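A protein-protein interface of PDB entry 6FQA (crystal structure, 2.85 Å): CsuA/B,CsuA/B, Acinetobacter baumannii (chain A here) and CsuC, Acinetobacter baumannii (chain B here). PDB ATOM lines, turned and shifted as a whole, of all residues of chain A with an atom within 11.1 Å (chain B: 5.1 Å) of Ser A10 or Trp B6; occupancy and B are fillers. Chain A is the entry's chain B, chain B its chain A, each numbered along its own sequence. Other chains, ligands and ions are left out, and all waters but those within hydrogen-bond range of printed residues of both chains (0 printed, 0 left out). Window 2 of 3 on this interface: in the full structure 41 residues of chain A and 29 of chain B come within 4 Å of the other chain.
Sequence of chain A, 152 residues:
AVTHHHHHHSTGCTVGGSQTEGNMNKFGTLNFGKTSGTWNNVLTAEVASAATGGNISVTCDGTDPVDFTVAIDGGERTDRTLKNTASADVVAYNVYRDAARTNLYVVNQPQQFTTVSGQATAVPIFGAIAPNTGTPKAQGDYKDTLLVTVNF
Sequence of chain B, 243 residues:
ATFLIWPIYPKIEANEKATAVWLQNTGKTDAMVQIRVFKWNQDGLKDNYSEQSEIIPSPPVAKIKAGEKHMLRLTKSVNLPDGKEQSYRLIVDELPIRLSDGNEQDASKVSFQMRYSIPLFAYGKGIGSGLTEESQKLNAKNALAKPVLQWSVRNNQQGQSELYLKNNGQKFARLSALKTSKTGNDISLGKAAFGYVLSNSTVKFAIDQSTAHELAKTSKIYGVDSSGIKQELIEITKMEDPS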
ATOM      1  N   HIS A   6       4.743  18.568  -7.587  1.00  0.00           N
ATOM      2  CA  HIS A   6       3.531  17.869  -7.156  1.00  0.00           C
ATOM      3  C   HIS A   6       2.462  17.736  -8.247  1.00  0.00           C
ATOM      4  O   HIS A   6       1.937  16.635  -8.421  1.00  0.00           O
ATOM      5  CB  HIS A   6       2.912  18.548  -5.927  1.00  0.00           C
ATOM      6  CG  HIS A   6       3.873  19.397  -5.153  1.00  0.00           C
ATOM      7  ND1 HIS A   6       4.924  18.868  -4.435  1.00  0.00           N
ATOM      8  CD2 HIS A   6       3.939  20.740  -4.984  1.00  0.00           C
ATOM      9  CE1 HIS A   6       5.599  19.848  -3.862  1.00  0.00           C
ATOM     10  NE2 HIS A   6       5.021  20.995  -4.177  1.00  0.00           N
ATOM     11  N   HIS A   7       2.102  18.799  -8.978  1.00  0.00           N
ATOM     12  CA  HIS A   7       2.652  20.162  -8.931  1.00  0.00           C
ATOM     13  C   HIS A   7       1.644  21.099  -8.253  1.00  0.00           C
ATOM     14  O   HIS A   7       1.637  21.292  -7.034  1.00  0.00           O
ATOM     15  CB  HIS A   7       2.969  20.628 -10.373  1.00  0.00           C
ATOM     16  CG  HIS A   7       3.590  21.993 -10.487  1.00  0.00           C
ATOM     17  ND1 HIS A   7       2.893  23.159 -10.242  1.00  0.00           N
ATOM     18  CD2 HIS A   7       4.824  22.377 -10.892  1.00  0.00           C
ATOM     19  CE1 HIS A   7       3.684  24.197 -10.450  1.00  0.00           C
ATOM     20  NE2 HIS A   7       4.861  23.750 -10.848  1.00  0.00           N
ATOM     21  N   HIS A   8       0.833  21.689  -9.117  1.00  0.00           N
ATOM     22  CA  HIS A   8      -0.393  22.428  -8.863  1.00  0.00           C
ATOM     23  C   HIS A   8      -1.551  21.440  -8.845  1.00  0.00           C
ATOM     24  O   HIS A   8      -1.409  20.289  -9.252  1.00  0.00           O
ATOM     25  CB  HIS A   8      -0.522  23.529  -9.939  1.00  0.00           C
ATOM     26  CG  HIS A   8      -1.902  23.742 -10.503  1.00  0.00           C
ATOM     27  ND1 HIS A   8      -2.903  24.412  -9.833  1.00  0.00           N
ATOM     28  CD2 HIS A   8      -2.408  23.446 -11.727  1.00  0.00           C
ATOM     29  CE1 HIS A   8      -3.978  24.481 -10.600  1.00  0.00           C
ATOM     30  NE2 HIS A   8      -3.703  23.904 -11.756  1.00  0.00           N
ATOM     31  N   HIS A   9      -2.695  21.872  -8.327  1.00  0.00           N
ATOM     32  CA  HIS A   9      -3.835  20.969  -8.226  1.00  0.00           C
ATOM     33  C   HIS A   9      -4.713  21.093  -9.462  1.00  0.00           C
ATOM     34  O   HIS A   9      -5.346  22.133  -9.678  1.00  0.00           O
ATOM     35  CB  HIS A   9      -4.695  21.262  -6.997  1.00  0.00           C
ATOM     36  CG  HIS A   9      -5.769  20.241  -6.783  1.00  0.00           C
ATOM     37  ND1 HIS A   9      -5.503  18.965  -6.336  1.00  0.00           N
ATOM     38  CD2 HIS A   9      -7.095  20.275  -7.060  1.00  0.00           C
ATOM     39  CE1 HIS A   9      -6.628  18.274  -6.290  1.00  0.00           C
ATOM     40  NE2 HIS A   9      -7.607  19.043  -6.732  1.00  0.00           N
ATOM     41  N   SER A  10      -4.821  20.006 -10.224  1.00  0.00           N
ATOM     42  CA  SER A  10      -5.765  19.993 -11.323  1.00  0.00           C
ATOM     43  C   SER A  10      -7.109  19.669 -10.707  1.00  0.00           C
ATOM     44  O   SER A  10      -7.351  18.537 -10.277  1.00  0.00           O
ATOM     45  CB  SER A  10      -5.370  18.984 -12.395  1.00  0.00           C
ATOM     46  OG  SER A  10      -4.206  19.392 -13.097  1.00  0.00           O
ATOM     47  N   THR A  11      -7.968  20.675 -10.638  1.00  0.00           N
ATOM     48  CA  THR A  11      -9.280  20.495 -10.054  1.00  0.00           C
ATOM     49  C   THR A  11     -10.127  19.624 -10.968  1.00  0.00           C
ATOM     50  O   THR A  11     -10.009  19.691 -12.193  1.00  0.00           O
ATOM     51  CB  THR A  11      -9.954  21.851  -9.812  1.00  0.00           C
ATOM     52  OG1 THR A  11      -9.003  22.782  -9.276  1.00  0.00           O
ATOM     53  CG2 THR A  11     -11.144  21.700  -8.871  1.00  0.00           C
ATOM     54  N   GLY A  12     -10.950  18.778 -10.357  1.00  0.00           N
ATOM     55  CA  GLY A  12     -11.934  17.978 -11.051  1.00  0.00           C
ATOM     56  C   GLY A  12     -13.240  17.975 -10.288  1.00  0.00           C
ATOM     57  O   GLY A  12     -13.221  18.023  -9.059  1.00  0.00           O
ATOM     58  N   CYS A  13     -14.376  17.999 -10.978  1.00  0.00           N
ATOM     59  CA  CYS A  13     -15.665  18.104 -10.307  1.00  0.00           C
ATOM     60  C   CYS A  13     -16.608  16.982 -10.719  1.00  0.00           C
ATOM     61  O   CYS A  13     -16.518  16.438 -11.820  1.00  0.00           O
ATOM     62  CB  CYS A  13     -16.313  19.452 -10.579  1.00  0.00           C
ATOM     63  SG  CYS A  13     -15.238  20.855 -10.196  1.00  0.00           S
ATOM     64  N   THR A  14     -17.522  16.654  -9.816  1.00  0.00           N
ATOM     65  CA  THR A  14     -18.574  15.672 -10.044  1.00  0.00           C
ATOM     66  C   THR A  14     -19.862  16.464 -10.181  1.00  0.00           C
ATOM     67  O   THR A  14     -20.378  17.005  -9.198  1.00  0.00           O
ATOM     68  CB  THR A  14     -18.639  14.656  -8.901  1.00  0.00           C
ATOM     69  OG1 THR A  14     -17.402  13.929  -8.808  1.00  0.00           O
ATOM     70  CG2 THR A  14     -19.777  13.692  -9.071  1.00  0.00           C
ATOM     71  N   VAL A  15     -20.330  16.575 -11.372  1.00  0.00           N
ATOM     72  CA  VAL A  15     -21.515  17.364 -11.660  1.00  0.00           C
ATOM     73  C   VAL A  15     -22.737  16.466 -11.677  1.00  0.00           C
ATOM     74  O   VAL A  15     -22.672  15.258 -11.953  1.00  0.00           O
ATOM     75  CB  VAL A  15     -21.355  18.113 -12.988  1.00  0.00           C
ATOM     76  CG1 VAL A  15     -20.241  19.108 -12.845  1.00  0.00           C
ATOM     77  CG2 VAL A  15     -21.101  17.123 -14.105  1.00  0.00           C
ATOM     78  N   THR A  59     -19.912  19.017  -7.085  1.00  0.00           N
ATOM     79  CA  THR A  59     -18.902  18.780  -6.057  1.00  0.00           C
ATOM     80  C   THR A  59     -17.520  18.819  -6.688  1.00  0.00           C
ATOM     81  O   THR A  59     -17.223  18.014  -7.576  1.00  0.00           O
ATOM     82  CB  THR A  59     -19.127  17.435  -5.372  1.00  0.00           C
ATOM     83  OG1 THR A  59     -20.371  17.466  -4.662  1.00  0.00           O
ATOM     84  CG2 THR A  59     -17.996  17.122  -4.427  1.00  0.00           C
ATOM     85  N   CYS A  60     -16.696  19.768  -6.258  1.00  0.00           N
ATOM     86  CA  CYS A  60     -15.319  19.903  -6.714  1.00  0.00           C
ATOM     87  C   CYS A  60     -14.365  19.497  -5.593  1.00  0.00           C
ATOM     88  O   CYS A  60     -14.771  19.239  -4.460  1.00  0.00           O
ATOM     89  CB  CYS A  60     -15.057  21.327  -7.195  1.00  0.00           C
ATOM     90  SG  CYS A  60     -16.085  21.759  -8.585  1.00  0.00           S
ATOM     91  N   ASP A  61     -13.072  19.479  -5.902  1.00  0.00           N
ATOM     92  CA  ASP A  61     -12.145  18.729  -5.074  1.00  0.00           C
ATOM     93  C   ASP A  61     -10.857  19.470  -4.724  1.00  0.00           C
ATOM     94  O   ASP A  61      -9.970  18.869  -4.100  1.00  0.00           O
ATOM     95  CB  ASP A  61     -11.813  17.407  -5.765  1.00  0.00           C
ATOM     96  CG  ASP A  61     -10.773  17.551  -6.867  1.00  0.00           C
ATOM     97  OD1 ASP A  61     -10.628  18.656  -7.441  1.00  0.00           O
ATOM     98  OD2 ASP A  61     -10.105  16.547  -7.164  1.00  0.00           O
ATOM     99  N   GLY A  62     -10.711  20.744  -5.071  1.00  0.00           N
ATOM    100  CA  GLY A  62      -9.525  21.457  -4.639  1.00  0.00           C
ATOM    101  C   GLY A  62      -9.530  21.739  -3.140  1.00  0.00           C
ATOM    102  O   GLY A  62     -10.289  21.168  -2.353  1.00  0.00           O
ATOM    103  N   THR A  63      -8.600  22.608  -2.741  1.00  0.00           N
ATOM    104  CA  THR A  63      -8.798  23.369  -1.515  1.00  0.00           C
ATOM    105  C   THR A  63      -9.508  24.678  -1.813  1.00  0.00           C
ATOM    106  O   THR A  63     -10.324  25.131  -1.004  1.00  0.00           O
ATOM    107  CB  THR A  63      -7.465  23.651  -0.819  1.00  0.00           C
ATOM    108  OG1 THR A  63      -6.587  24.339  -1.716  1.00  0.00           O
ATOM    109  CG2 THR A  63      -6.816  22.348  -0.394  1.00  0.00           C
ATOM    110  N   ASP A  64      -9.265  25.244  -2.999  1.00  0.00           N
ATOM    111  CA  ASP A  64      -9.909  26.474  -3.418  1.00  0.00           C
ATOM    112  C   ASP A  64     -11.389  26.240  -3.679  1.00  0.00           C
ATOM    113  O   ASP A  64     -11.817  25.114  -3.928  1.00  0.00           O
ATOM    114  CB  ASP A  64      -9.281  27.005  -4.707  1.00  0.00           C
ATOM    115  CG  ASP A  64      -7.841  27.421  -4.543  1.00  0.00           C
ATOM    116  OD1 ASP A  64      -7.341  27.403  -3.401  1.00  0.00           O
ATOM    117  OD2 ASP A  64      -7.212  27.774  -5.565  1.00  0.00           O
ATOM    118  N   PRO A  65     -12.196  27.292  -3.638  1.00  0.00           N
ATOM    119  CA  PRO A  65     -13.555  27.184  -4.167  1.00  0.00           C
ATOM    120  C   PRO A  65     -13.497  27.283  -5.679  1.00  0.00           C
ATOM    121  O   PRO A  65     -12.533  27.784  -6.260  1.00  0.00           O
ATOM    122  CB  PRO A  65     -14.296  28.383  -3.557  1.00  0.00           C
ATOM    123  CG  PRO A  65     -13.236  29.215  -2.845  1.00  0.00           C
ATOM    124  CD  PRO A  65     -11.884  28.673  -3.220  1.00  0.00           C
ATOM    125  N   VAL A  66     -14.530  26.755  -6.319  1.00  0.00           N
ATOM    126  CA  VAL A  66     -14.690  26.864  -7.763  1.00  0.00           C
ATOM    127  C   VAL A  66     -15.977  27.617  -8.037  1.00  0.00           C
ATOM    128  O   VAL A  66     -17.042  27.189  -7.593  1.00  0.00           O
ATOM    129  CB  VAL A  66     -14.699  25.488  -8.436  1.00  0.00           C
ATOM    130  CG1 VAL A  66     -15.053  25.646  -9.893  1.00  0.00           C
ATOM    131  CG2 VAL A  66     -13.333  24.822  -8.278  1.00  0.00           C
ATOM    132  N   PHE A 152     -18.286  25.945 -16.079  1.00  0.00           N
ATOM    133  CA  PHE A 152     -17.140  26.253 -15.231  1.00  0.00           C
ATOM    134  C   PHE A 152     -16.157  27.246 -15.849  1.00  0.00           C
ATOM    135  O   PHE A 152     -15.292  27.816 -15.152  1.00  0.00           O
ATOM    136  CB  PHE A 152     -16.384  24.971 -14.900  1.00  0.00           C
ATOM    137  CG  PHE A 152     -17.199  23.969 -14.193  1.00  0.00           C
ATOM    138  CD1 PHE A 152     -17.324  24.011 -12.829  1.00  0.00           C
ATOM    139  CD2 PHE A 152     -17.851  22.974 -14.892  1.00  0.00           C
ATOM    140  CE1 PHE A 152     -18.081  23.089 -12.174  1.00  0.00           C
ATOM    141  CE2 PHE A 152     -18.609  22.057 -14.241  1.00  0.00           C
ATOM    142  CZ  PHE A 152     -18.728  22.115 -12.876  1.00  0.00           C
ATOM    143  OXT PHE A 152     -16.237  27.518 -17.047  1.00  0.00           O
ATOM    144  N   LEU B   4     -18.023  12.657 -13.292  1.00  0.00           N
ATOM    145  CA  LEU B   4     -16.794  13.244 -12.764  1.00  0.00           C
ATOM    146  C   LEU B   4     -15.961  13.704 -13.950  1.00  0.00           C
ATOM    147  O   LEU B   4     -15.519  12.877 -14.750  1.00  0.00           O
ATOM    148  CB  LEU B   4     -16.005  12.244 -11.917  1.00  0.00           C
ATOM    149  CG  LEU B   4     -14.607  12.740 -11.513  1.00  0.00           C
ATOM    150  CD1 LEU B   4     -14.702  13.955 -10.639  1.00  0.00           C
ATOM    151  CD2 LEU B   4     -13.789  11.684 -10.817  1.00  0.00           C
ATOM    152  N   ILE B   5     -15.761  15.016 -14.080  1.00  0.00           N
ATOM    153  CA  ILE B   5     -14.955  15.595 -15.161  1.00  0.00           C
ATOM    154  C   ILE B   5     -13.637  16.074 -14.568  1.00  0.00           C
ATOM    155  O   ILE B   5     -13.630  16.755 -13.533  1.00  0.00           O
ATOM    156  CB  ILE B   5     -15.677  16.759 -15.862  1.00  0.00           C
ATOM    157  CG1 ILE B   5     -17.107  16.383 -16.252  1.00  0.00           C
ATOM    158  CG2 ILE B   5     -14.904  17.193 -17.080  1.00  0.00           C
ATOM    159  CD1 ILE B   5     -17.954  17.580 -16.502  1.00  0.00           C
ATOM    160  N   TRP B   6     -12.521  15.720 -15.222  1.00  0.00           N
ATOM    161  CA  TRP B   6     -11.173  16.038 -14.746  1.00  0.00           C
ATOM    162  C   TRP B   6     -10.259  16.050 -15.957  1.00  0.00           C
ATOM    163  O   TRP B   6     -10.302  15.100 -16.750  1.00  0.00           O
ATOM    164  CB  TRP B   6     -10.637  15.034 -13.722  1.00  0.00           C
ATOM    165  CG  TRP B   6      -9.231  15.331 -13.305  1.00  0.00           C
ATOM    166  CD1 TRP B   6      -8.828  16.159 -12.287  1.00  0.00           C
ATOM    167  CD2 TRP B   6      -8.029  14.835 -13.908  1.00  0.00           C
ATOM    168  NE1 TRP B   6      -7.452  16.203 -12.215  1.00  0.00           N
ATOM    169  CE2 TRP B   6      -6.937  15.404 -13.199  1.00  0.00           C
ATOM    170  CE3 TRP B   6      -7.762  13.969 -14.977  1.00  0.00           C
ATOM    171  CZ2 TRP B   6      -5.612  15.133 -13.524  1.00  0.00           C
ATOM    172  CZ3 TRP B   6      -6.441  13.706 -15.300  1.00  0.00           C
ATOM    173  CH2 TRP B   6      -5.382  14.281 -14.571  1.00  0.00           C
ATOM    174  N   PRO B   7      -9.437  17.084 -16.136  1.00  0.00           N
ATOM    175  CA  PRO B   7      -9.440  18.341 -15.408  1.00  0.00           C
ATOM    176  C   PRO B   7     -10.488  19.318 -15.906  1.00  0.00           C
ATOM    177  O   PRO B   7     -10.750  19.423 -17.103  1.00  0.00           O
ATOM    178  CB  PRO B   7      -8.054  18.894 -15.699  1.00  0.00           C
ATOM    179  CG  PRO B   7      -7.794  18.444 -17.039  1.00  0.00           C
ATOM    180  CD  PRO B   7      -8.270  17.019 -17.030  1.00  0.00           C
ATOM    181  N   ILE B   8     -11.036  20.066 -14.951  1.00  0.00           N
ATOM    182  CA  ILE B   8     -12.008  21.101 -15.249  1.00  0.00           C
ATOM    183  C   ILE B   8     -11.375  22.296 -15.972  1.00  0.00           C
ATOM    184  O   ILE B   8     -12.065  23.011 -16.701  1.00  0.00           O
ATOM    185  CB  ILE B   8     -12.732  21.426 -13.918  1.00  0.00           C
ATOM    186  CG1 ILE B   8     -14.233  21.293 -14.097  1.00  0.00           C
ATOM    187  CG2 ILE B   8     -12.377  22.795 -13.341  1.00  0.00           C
ATOM    188  CD1 ILE B   8     -14.669  19.873 -14.354  1.00  0.00           C
ATOM    189  N   ALA B  20      -5.957  15.557 -22.881  1.00  0.00           N
ATOM    190  CA  ALA B  20      -7.034  14.658 -22.536  1.00  0.00           C
ATOM    191  C   ALA B  20      -7.879  15.290 -21.451  1.00  0.00           C
ATOM    192  O   ALA B  20      -7.367  15.975 -20.559  1.00  0.00           O
ATOM    193  CB  ALA B  20      -6.500  13.327 -22.060  1.00  0.00           C
ATOM    194  N   VAL B  21      -9.177  15.084 -21.561  1.00  0.00           N
ATOM    195  CA  VAL B  21     -10.104  15.310 -20.469  1.00  0.00           C
ATOM    196  C   VAL B  21     -10.751  13.974 -20.155  1.00  0.00           C
ATOM    197  O   VAL B  21     -11.089  13.205 -21.063  1.00  0.00           O
ATOM    198  CB  VAL B  21     -11.154  16.371 -20.825  1.00  0.00           C
ATOM    199  CG1 VAL B  21     -12.131  16.512 -19.690  1.00  0.00           C
ATOM    200  CG2 VAL B  21     -10.463  17.694 -21.112  1.00  0.00           C
ATOM    201  N   TRP B  22     -10.870  13.665 -18.875  1.00  0.00           N
ATOM    202  CA  TRP B  22     -11.440  12.391 -18.493  1.00  0.00           C
ATOM    203  C   TRP B  22     -12.882  12.595 -18.076  1.00  0.00           C
ATOM    204  O   TRP B  22     -13.234  13.601 -17.461  1.00  0.00           O
ATOM    205  CB  TRP B  22     -10.615  11.722 -17.389  1.00  0.00           C
ATOM    206  CG  TRP B  22      -9.464  10.901 -17.955  1.00  0.00           C
ATOM    207  CD1 TRP B  22      -9.489   9.567 -18.313  1.00  0.00           C
ATOM    208  CD2 TRP B  22      -8.150  11.371 -18.272  1.00  0.00           C
ATOM    209  NE1 TRP B  22      -8.263   9.190 -18.818  1.00  0.00           N
ATOM    210  CE2 TRP B  22      -7.424  10.276 -18.795  1.00  0.00           C
ATOM    211  CE3 TRP B  22      -7.511  12.607 -18.152  1.00  0.00           C
ATOM    212  CZ2 TRP B  22      -6.087  10.388 -19.190  1.00  0.00           C
ATOM    213  CZ3 TRP B  22      -6.175  12.712 -18.537  1.00  0.00           C
ATOM    214  CH2 TRP B  22      -5.483  11.611 -19.051  1.00  0.00           C
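Ser A10 touches just one residue of chain B: Trp B6. Printed residues of chain B within 4 Å of Thr A11: Trp B6, Pro B7 and Ile B8. Printed residues of chain B within 4 Å of Gly A12: Ile B5 (3.2 Å) and Trp B6 (3.8 Å). Of the printed residues of chain B, Cys A13 touches Leu B4 (3.3 Å), Ile B5 (2.8 Å) and Ile B8 (3.9 Å). Of the printed residues of chain B, Thr A14 touches Leu B4. Asp A64 touches none of the printed residues of chain B. Pro A65 touches none of the printed residues of chain B. Pro B7 touches just one residue of chain A: Thr A11. Of the printed residues of chain A, Ile B8 touches Thr A11, Cys A13 and Phe A152. No residue of chain A comes within 4 Å of Trp B22. The nearest printed residue of chain B that does not touch Val A15 is Leu B4 (4.9 Å).
O of Cys A13 sits at hydrogen-bond distance from N of Ile B5, 2.8 Å away. The backbone carbonyl oxygen (O) of Ser A10 is in hydrogen-bond range of the indole nitrogen (NE1) of Trp B6 (3.0 Å). The backbone NH (N) of Ile B8 sits at hydrogen-bond distance from the backbone carbonyl oxygen (O) of Thr A11 (3.0 Å).
Hydrophobic or aromatic side chains of chain A that line the printed part of chain B: Val A15 and Phe A152. Printed residues of chain B that touch a printed residue of chain A: Leu B4, Ile B5, Trp B6, Pro B7 and Ile B8. Hydrophobic or aromatic side chains of chain B that line the printed part of chain A: Leu B4, Ile B5, Trp B6 and Ile B8. Among the printed residues, no Asp or Glu carboxylate lies within 4 Å of a Lys or Arg side-chain nitrogen of the other chain.
Among the printed residues, pairs that only touch across the chains: Gly A12 with Ile B5, Thr A14 with Leu B4, Cys A13 with Leu B4, Thr A11 with Pro B7, Thr A11 with Trp B6, Gly A12 with Trp B6, Cys A13 with Ile B8, Val A15 with Ile B5 and Phe A152 with Ile B8.
The backbone carbonyl oxygen of Trp B6 sits at hydrogen-bond distance from the backbone NH of Trp B22 (2.6 Å). The side-chain carboxylate (OD1) of Asp A61 is in hydrogen-bond range of the backbone NH (N) of Gly A12, 2.9 Å away. The side-chain sulfur of Cys A13 forms a disulfide with the side-chain sulfur of Cys A60 (2.0 Å). N of Thr A14 is in hydrogen-bond range of O of Thr A59, 2.6 Å away.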
